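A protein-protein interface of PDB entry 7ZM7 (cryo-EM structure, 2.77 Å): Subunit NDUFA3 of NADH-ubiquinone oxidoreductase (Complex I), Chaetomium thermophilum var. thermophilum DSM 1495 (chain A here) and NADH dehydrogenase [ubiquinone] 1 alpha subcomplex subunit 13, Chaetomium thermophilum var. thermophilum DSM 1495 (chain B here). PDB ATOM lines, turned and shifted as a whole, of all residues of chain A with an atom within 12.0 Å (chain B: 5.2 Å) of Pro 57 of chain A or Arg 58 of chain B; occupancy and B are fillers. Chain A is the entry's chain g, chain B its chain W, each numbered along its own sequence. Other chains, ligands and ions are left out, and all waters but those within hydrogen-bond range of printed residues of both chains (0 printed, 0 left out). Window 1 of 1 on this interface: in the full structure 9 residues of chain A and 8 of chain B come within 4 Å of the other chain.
The backbone carbonyl oxygen of Pro 57 of chain A lies within hydrogen-bond range of the guanidinium group of Arg 58 of chain B.
NH1 of Arg 58 of chain B is in hydrogen-bond range of O of Ala 56 of chain A (2.8 Å).
NE of Arg 58 of chain B lies within salt-bridge range of OE1 of Glu 55 of chain B.
Glu 55 of chain B touches Ala 55 of chain A (OE2 to CB, 3.9 Å).
Ile 58 of chain A touches Asn 54 of chain B (CG2 to O, 3.8 Å).
Met 61 of chain B touches Ile 58 of chain A (CG to CD1, 3.96 Å).
O of Pro 59 of chain A touches CG of Met 61 of chain B, 3.4 Å away.
CG of Pro 59 of chain A touches NE1 of Trp 62 of chain B, 3.7 Å away.
CG of Pro 63 of chain A touches CH2 of Trp 62 of chain B, 3.5 Å away.
Of chain B, only Arg 58 (3.2 Å) comes within 4 Å of Pro 57 of chain A.
Arg 58 of chain B touches just these residues of chain A: Ala 56 (2.8 Å) and Pro 57 (3.2 Å).
Of chain A, only Ala 55 comes within 4 Å of Glu 55 of chain B.
No residue of chain A comes within 4 Å of Ala 57 of chain B.
No residue of chain A comes within 4 Å of Glu 59 of chain B.
Met 61 of chain B touches just these residues of chain A: Ile 58 and Pro 59.
Printed residues of chain B within 4 Å of Ile 58 of chain A: Asn 54 (3.8 Å) and Met 61 (3.96 Å).
Of the printed residues of chain B, Pro 63 of chain A touches Trp 62.
Lys 60 of chain B touches none of the printed residues of chain A.
The nearest printed residue of chain B that does not touch Ile 58 of chain A is Ala 57 of chain B (4.1 Å).
Of the 10 printed residues of chain B, 5 touch a printed residue of chain A.
Printed residues of chain B that touch a printed residue of chain A: Asn 54, Glu 55, Arg 58, Met 61 and Trp 62.
Of the 12 printed residues of chain A, 6 touch a printed residue of chain B.
Hydrophobic or aromatic side chains of chain A that line the printed part of chain B: Ala 55, Ala 56, Ile 58, Pro 59 and Pro 63.
Along chain A the printed residues that touch a printed residue of chain B span positions 55 to 63.
Among the printed residues, 8 pairs touch across the chains.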
ATOM      1  N   ARG A  47     -31.315  22.379  11.322  1.00  0.00           N
ATOM      2  CA  ARG A  47     -29.925  22.903  11.359  1.00  0.00           C
ATOM      3  C   ARG A  47     -29.290  22.786   9.964  1.00  0.00           C
ATOM      4  O   ARG A  47     -28.606  23.732   9.555  1.00  0.00           O
ATOM      5  CB  ARG A  47     -29.099  22.178  12.426  1.00  0.00           C
ATOM      6  CG  ARG A  47     -29.042  22.909  13.758  1.00  0.00           C
ATOM      7  CD  ARG A  47     -28.104  22.291  14.775  1.00  0.00           C
ATOM      8  NE  ARG A  47     -26.702  22.262  14.381  1.00  0.00           N
ATOM      9  CZ  ARG A  47     -26.013  21.164  14.085  1.00  0.00           C
ATOM     10  NH1 ARG A  47     -24.742  21.257  13.739  1.00  0.00           N
ATOM     11  NH2 ARG A  47     -26.591  19.979  14.140  1.00  0.00           N
ATOM     12  N   VAL A  53     -23.561  23.599   9.515  1.00  0.00           N
ATOM     13  CA  VAL A  53     -22.870  22.302   9.246  1.00  0.00           C
ATOM     14  C   VAL A  53     -22.204  21.795  10.524  1.00  0.00           C
ATOM     15  O   VAL A  53     -21.619  22.616  11.253  1.00  0.00           O
ATOM     16  CB  VAL A  53     -21.864  22.426   8.083  1.00  0.00           C
ATOM     17  CG1 VAL A  53     -22.567  22.446   6.736  1.00  0.00           C
ATOM     18  CG2 VAL A  53     -20.959  23.639   8.233  1.00  0.00           C
ATOM     19  N   ASP A  54     -22.306  20.490  10.786  1.00  0.00           N
ATOM     20  CA  ASP A  54     -21.637  19.893  11.972  1.00  0.00           C
ATOM     21  C   ASP A  54     -20.124  20.029  11.800  1.00  0.00           C
ATOM     22  O   ASP A  54     -19.635  19.798  10.678  1.00  0.00           O
ATOM     23  CB  ASP A  54     -22.035  18.430  12.176  1.00  0.00           C
ATOM     24  CG  ASP A  54     -23.513  18.228  12.462  1.00  0.00           C
ATOM     25  OD1 ASP A  54     -24.334  18.952  11.863  1.00  0.00           O
ATOM     26  OD2 ASP A  54     -23.834  17.352  13.288  1.00  0.00           O
ATOM     27  N   ALA A  55     -19.417  20.369  12.879  1.00  0.00           N
ATOM     28  CA  ALA A  55     -17.949  20.536  12.826  1.00  0.00           C
ATOM     29  C   ALA A  55     -17.286  19.211  12.460  1.00  0.00           C
ATOM     30  O   ALA A  55     -17.805  18.160  12.882  1.00  0.00           O
ATOM     31  CB  ALA A  55     -17.456  21.010  14.167  1.00  0.00           C
ATOM     32  N   ALA A  56     -16.174  19.258  11.724  1.00  0.00           N
ATOM     33  CA  ALA A  56     -15.417  18.021  11.429  1.00  0.00           C
ATOM     34  C   ALA A  56     -14.916  17.402  12.737  1.00  0.00           C
ATOM     35  O   ALA A  56     -14.693  18.169  13.678  1.00  0.00           O
ATOM     36  CB  ALA A  56     -14.265  18.321  10.508  1.00  0.00           C
ATOM     37  N   PRO A  57     -14.724  16.065  12.873  1.00  0.00           N
ATOM     38  CA  PRO A  57     -14.148  15.523  14.097  1.00  0.00           C
ATOM     39  C   PRO A  57     -12.697  15.975  14.330  1.00  0.00           C
ATOM     40  O   PRO A  57     -11.990  16.264  13.389  1.00  0.00           O
ATOM     41  CB  PRO A  57     -14.345  14.011  13.947  1.00  0.00           C
ATOM     42  CG  PRO A  57     -14.430  13.792  12.458  1.00  0.00           C
ATOM     43  CD  PRO A  57     -15.133  15.024  11.933  1.00  0.00           C
ATOM     44  N   ILE A  58     -12.327  16.102  15.603  1.00  0.00           N
ATOM     45  CA  ILE A  58     -10.938  16.503  15.936  1.00  0.00           C
ATOM     46  C   ILE A  58     -10.063  15.262  15.781  1.00  0.00           C
ATOM     47  O   ILE A  58     -10.624  14.164  15.935  1.00  0.00           O
ATOM     48  CB  ILE A  58     -10.824  17.171  17.316  1.00  0.00           C
ATOM     49  CG1 ILE A  58     -10.950  16.165  18.461  1.00  0.00           C
ATOM     50  CG2 ILE A  58     -11.815  18.316  17.439  1.00  0.00           C
ATOM     51  CD1 ILE A  58     -10.181  16.558  19.694  1.00  0.00           C
ATOM     52  N   PRO A  59      -8.751  15.350  15.428  1.00  0.00           N
ATOM     53  CA  PRO A  59      -7.902  14.157  15.382  1.00  0.00           C
ATOM     54  C   PRO A  59      -7.613  13.593  16.765  1.00  0.00           C
ATOM     55  O   PRO A  59      -7.354  14.325  17.716  1.00  0.00           O
ATOM     56  CB  PRO A  59      -6.629  14.670  14.716  1.00  0.00           C
ATOM     57  CG  PRO A  59      -6.643  16.128  14.978  1.00  0.00           C
ATOM     58  CD  PRO A  59      -8.050  16.540  14.930  1.00  0.00           C
ATOM     59  N   LEU A  60      -7.677  12.279  16.909  1.00  0.00           N
ATOM     60  CA  LEU A  60      -7.365  11.633  18.205  1.00  0.00           C
ATOM     61  C   LEU A  60      -6.279  10.591  17.961  1.00  0.00           C
ATOM     62  O   LEU A  60      -6.034   9.801  18.866  1.00  0.00           O
ATOM     63  CB  LEU A  60      -8.630  11.027  18.819  1.00  0.00           C
ATOM     64  CG  LEU A  60      -9.718  12.018  19.221  1.00  0.00           C
ATOM     65  CD1 LEU A  60     -11.012  11.298  19.551  1.00  0.00           C
ATOM     66  CD2 LEU A  60      -9.272  12.871  20.393  1.00  0.00           C
ATOM     67  N   THR A  61      -5.654  10.612  16.789  1.00  0.00           N
ATOM     68  CA  THR A  61      -4.510   9.731  16.466  1.00  0.00           C
ATOM     69  C   THR A  61      -3.658  10.539  15.495  1.00  0.00           C
ATOM     70  O   THR A  61      -4.171  11.552  14.997  1.00  0.00           O
ATOM     71  CB  THR A  61      -4.950   8.367  15.910  1.00  0.00           C
ATOM     72  OG1 THR A  61      -3.863   7.448  15.960  1.00  0.00           O
ATOM     73  CG2 THR A  61      -5.489   8.414  14.501  1.00  0.00           C
ATOM     74  N   TYR A  62      -2.434  10.109  15.219  1.00  0.00           N
ATOM     75  CA  TYR A  62      -1.602  10.814  14.216  1.00  0.00           C
ATOM     76  C   TYR A  62      -2.288  10.776  12.848  1.00  0.00           C
ATOM     77  O   TYR A  62      -2.659   9.678  12.416  1.00  0.00           O
ATOM     78  CB  TYR A  62      -0.144  10.346  14.154  1.00  0.00           C
ATOM     79  CG  TYR A  62       0.696  11.166  13.209  1.00  0.00           C
ATOM     80  CD1 TYR A  62       0.742  10.875  11.857  1.00  0.00           C
ATOM     81  CD2 TYR A  62       1.419  12.256  13.657  1.00  0.00           C
ATOM     82  CE1 TYR A  62       1.479  11.641  10.975  1.00  0.00           C
ATOM     83  CE2 TYR A  62       2.180  13.022  12.792  1.00  0.00           C
ATOM     84  CZ  TYR A  62       2.202  12.719  11.444  1.00  0.00           C
ATOM     85  OH  TYR A  62       2.941  13.469  10.581  1.00  0.00           O
ATOM     86  N   PRO A  63      -2.439  11.919  12.120  1.00  0.00           N
ATOM     87  CA  PRO A  63      -3.164  11.877  10.870  1.00  0.00           C
ATOM     88  C   PRO A  63      -2.286  11.464   9.700  1.00  0.00           C
ATOM     89  O   PRO A  63      -1.715  12.325   9.065  1.00  0.00           O
ATOM     90  CB  PRO A  63      -3.568  13.327  10.712  1.00  0.00           C
ATOM     91  CG  PRO A  63      -2.450  14.110  11.349  1.00  0.00           C
ATOM     92  CD  PRO A  63      -1.992  13.250  12.498  1.00  0.00           C
ATOM     93  N   ASN B  54     -14.334  23.026  21.472  1.00  0.00           N
ATOM     94  CA  ASN B  54     -14.010  21.954  20.501  1.00  0.00           C
ATOM     95  C   ASN B  54     -12.975  22.462  19.498  1.00  0.00           C
ATOM     96  O   ASN B  54     -12.118  21.675  19.104  1.00  0.00           O
ATOM     97  CB  ASN B  54     -15.299  21.409  19.895  1.00  0.00           C
ATOM     98  CG  ASN B  54     -16.067  20.508  20.836  1.00  0.00           C
ATOM     99  OD1 ASN B  54     -15.502  19.967  21.779  1.00  0.00           O
ATOM    100  ND2 ASN B  54     -17.351  20.328  20.584  1.00  0.00           N
ATOM    101  N   GLU B  55     -13.091  23.714  19.072  1.00  0.00           N
ATOM    102  CA  GLU B  55     -12.118  24.340  18.142  1.00  0.00           C
ATOM    103  C   GLU B  55     -10.755  24.551  18.816  1.00  0.00           C
ATOM    104  O   GLU B  55      -9.728  24.422  18.130  1.00  0.00           O
ATOM    105  CB  GLU B  55     -12.770  25.549  17.470  1.00  0.00           C
ATOM    106  CG  GLU B  55     -13.893  25.167  16.529  1.00  0.00           C
ATOM    107  CD  GLU B  55     -13.630  23.898  15.736  1.00  0.00           C
ATOM    108  OE1 GLU B  55     -12.553  23.800  15.112  1.00  0.00           O
ATOM    109  OE2 GLU B  55     -14.502  23.007  15.747  1.00  0.00           O
ATOM    110  N   LEU B  56     -10.741  24.900  20.101  1.00  0.00           N
ATOM    111  CA  LEU B  56      -9.460  25.013  20.846  1.00  0.00           C
ATOM    112  C   LEU B  56      -8.803  23.638  20.908  1.00  0.00           C
ATOM    113  O   LEU B  56      -7.576  23.567  20.804  1.00  0.00           O
ATOM    114  CB  LEU B  56      -9.720  25.594  22.237  1.00  0.00           C
ATOM    115  CG  LEU B  56     -10.129  27.062  22.271  1.00  0.00           C
ATOM    116  CD1 LEU B  56     -10.554  27.470  23.671  1.00  0.00           C
ATOM    117  CD2 LEU B  56      -9.002  27.943  21.766  1.00  0.00           C
ATOM    118  N   ALA B  57      -9.596  22.588  21.076  1.00  0.00           N
ATOM    119  CA  ALA B  57      -9.065  21.210  21.073  1.00  0.00           C
ATOM    120  C   ALA B  57      -8.459  20.825  19.712  1.00  0.00           C
ATOM    121  O   ALA B  57      -7.450  20.117  19.712  1.00  0.00           O
ATOM    122  CB  ALA B  57     -10.108  20.239  21.555  1.00  0.00           C
ATOM    123  N   ARG B  58      -9.045  21.260  18.601  1.00  0.00           N
ATOM    124  CA  ARG B  58      -8.457  20.968  17.270  1.00  0.00           C
ATOM    125  C   ARG B  58      -7.060  21.586  17.172  1.00  0.00           C
ATOM    126  O   ARG B  58      -6.166  20.908  16.655  1.00  0.00           O
ATOM    127  CB  ARG B  58      -9.374  21.446  16.147  1.00  0.00           C
ATOM    128  CG  ARG B  58      -8.980  20.937  14.769  1.00  0.00           C
ATOM    129  CD  ARG B  58      -9.814  21.556  13.668  1.00  0.00           C
ATOM    130  NE  ARG B  58     -11.227  21.508  13.995  1.00  0.00           N
ATOM    131  CZ  ARG B  58     -12.035  20.497  13.711  1.00  0.00           C
ATOM    132  NH1 ARG B  58     -13.307  20.557  14.059  1.00  0.00           N
ATOM    133  NH2 ARG B  58     -11.571  19.432  13.085  1.00  0.00           N
ATOM    134  N   GLU B  59      -6.890  22.808  17.680  1.00  0.00           N
ATOM    135  CA  GLU B  59      -5.577  23.501  17.666  1.00  0.00           C
ATOM    136  C   GLU B  59      -4.597  22.781  18.594  1.00  0.00           C
ATOM    137  O   GLU B  59      -3.458  22.560  18.172  1.00  0.00           O
ATOM    138  CB  GLU B  59      -5.767  24.940  18.140  1.00  0.00           C
ATOM    139  CG  GLU B  59      -4.494  25.762  18.175  1.00  0.00           C
ATOM    140  CD  GLU B  59      -4.722  27.198  18.608  1.00  0.00           C
ATOM    141  OE1 GLU B  59      -3.795  28.016  18.458  1.00  0.00           O
ATOM    142  OE2 GLU B  59      -5.828  27.494  19.097  1.00  0.00           O
ATOM    143  N   LYS B  60      -5.033  22.429  19.802  1.00  0.00           N
ATOM    144  CA  LYS B  60      -4.164  21.685  20.743  1.00  0.00           C
ATOM    145  C   LYS B  60      -3.671  20.398  20.089  1.00  0.00           C
ATOM    146  O   LYS B  60      -2.472  20.121  20.207  1.00  0.00           O
ATOM    147  CB  LYS B  60      -4.892  21.406  22.059  1.00  0.00           C
ATOM    148  CG  LYS B  60      -4.003  20.977  23.215  1.00  0.00           C
ATOM    149  CD  LYS B  60      -4.750  20.291  24.332  1.00  0.00           C
ATOM    150  CE  LYS B  60      -4.259  20.694  25.704  1.00  0.00           C
ATOM    151  NZ  LYS B  60      -4.572  22.112  25.998  1.00  0.00           N
ATOM    152  N   MET B  61      -4.547  19.640  19.438  1.00  0.00           N
ATOM    153  CA  MET B  61      -4.161  18.333  18.864  1.00  0.00           C
ATOM    154  C   MET B  61      -3.208  18.568  17.697  1.00  0.00           C
ATOM    155  O   MET B  61      -2.179  17.909  17.648  1.00  0.00           O
ATOM    156  CB  MET B  61      -5.373  17.518  18.401  1.00  0.00           C
ATOM    157  CG  MET B  61      -6.248  17.006  19.527  1.00  0.00           C
ATOM    158  SD  MET B  61      -5.422  15.828  20.627  1.00  0.00           S
ATOM    159  CE  MET B  61      -4.671  16.937  21.815  1.00  0.00           C
ATOM    160  N   TRP B  62      -3.534  19.511  16.816  1.00  0.00           N
ATOM    161  CA  TRP B  62      -2.666  19.748  15.675  1.00  0.00           C
ATOM    162  C   TRP B  62      -1.325  20.316  16.102  1.00  0.00           C
ATOM    163  O   TRP B  62      -0.319  20.097  15.429  1.00  0.00           O
ATOM    164  CB  TRP B  62      -3.364  20.674  14.683  1.00  0.00           C
ATOM    165  CG  TRP B  62      -4.277  19.920  13.787  1.00  0.00           C
ATOM    166  CD1 TRP B  62      -5.630  19.919  13.806  1.00  0.00           C
ATOM    167  CD2 TRP B  62      -3.890  19.021  12.749  1.00  0.00           C
ATOM    168  NE1 TRP B  62      -6.116  19.084  12.840  1.00  0.00           N
ATOM    169  CE2 TRP B  62      -5.063  18.522  12.175  1.00  0.00           C
ATOM    170  CE3 TRP B  62      -2.663  18.605  12.243  1.00  0.00           C
ATOM    171  CZ2 TRP B  62      -5.044  17.631  11.129  1.00  0.00           C
ATOM    172  CZ3 TRP B  62      -2.651  17.728  11.215  1.00  0.00           C
ATOM    173  CH2 TRP B  62      -3.827  17.242  10.665  1.00  0.00           C
ATOM    174  N   ALA B  63      -1.265  20.975  17.255  1.00  0.00           N
ATOM    175  CA  ALA B  63       0.016  21.488  17.783  1.00  0.00           C
ATOM    176  C   ALA B  63       0.866  20.313  18.273  1.00  0.00           C
ATOM    177  O   ALA B  63       2.069  20.295  17.970  1.00  0.00           O
ATOM    178  CB  ALA B  63      -0.271  22.464  18.883  1.00  0.00           C
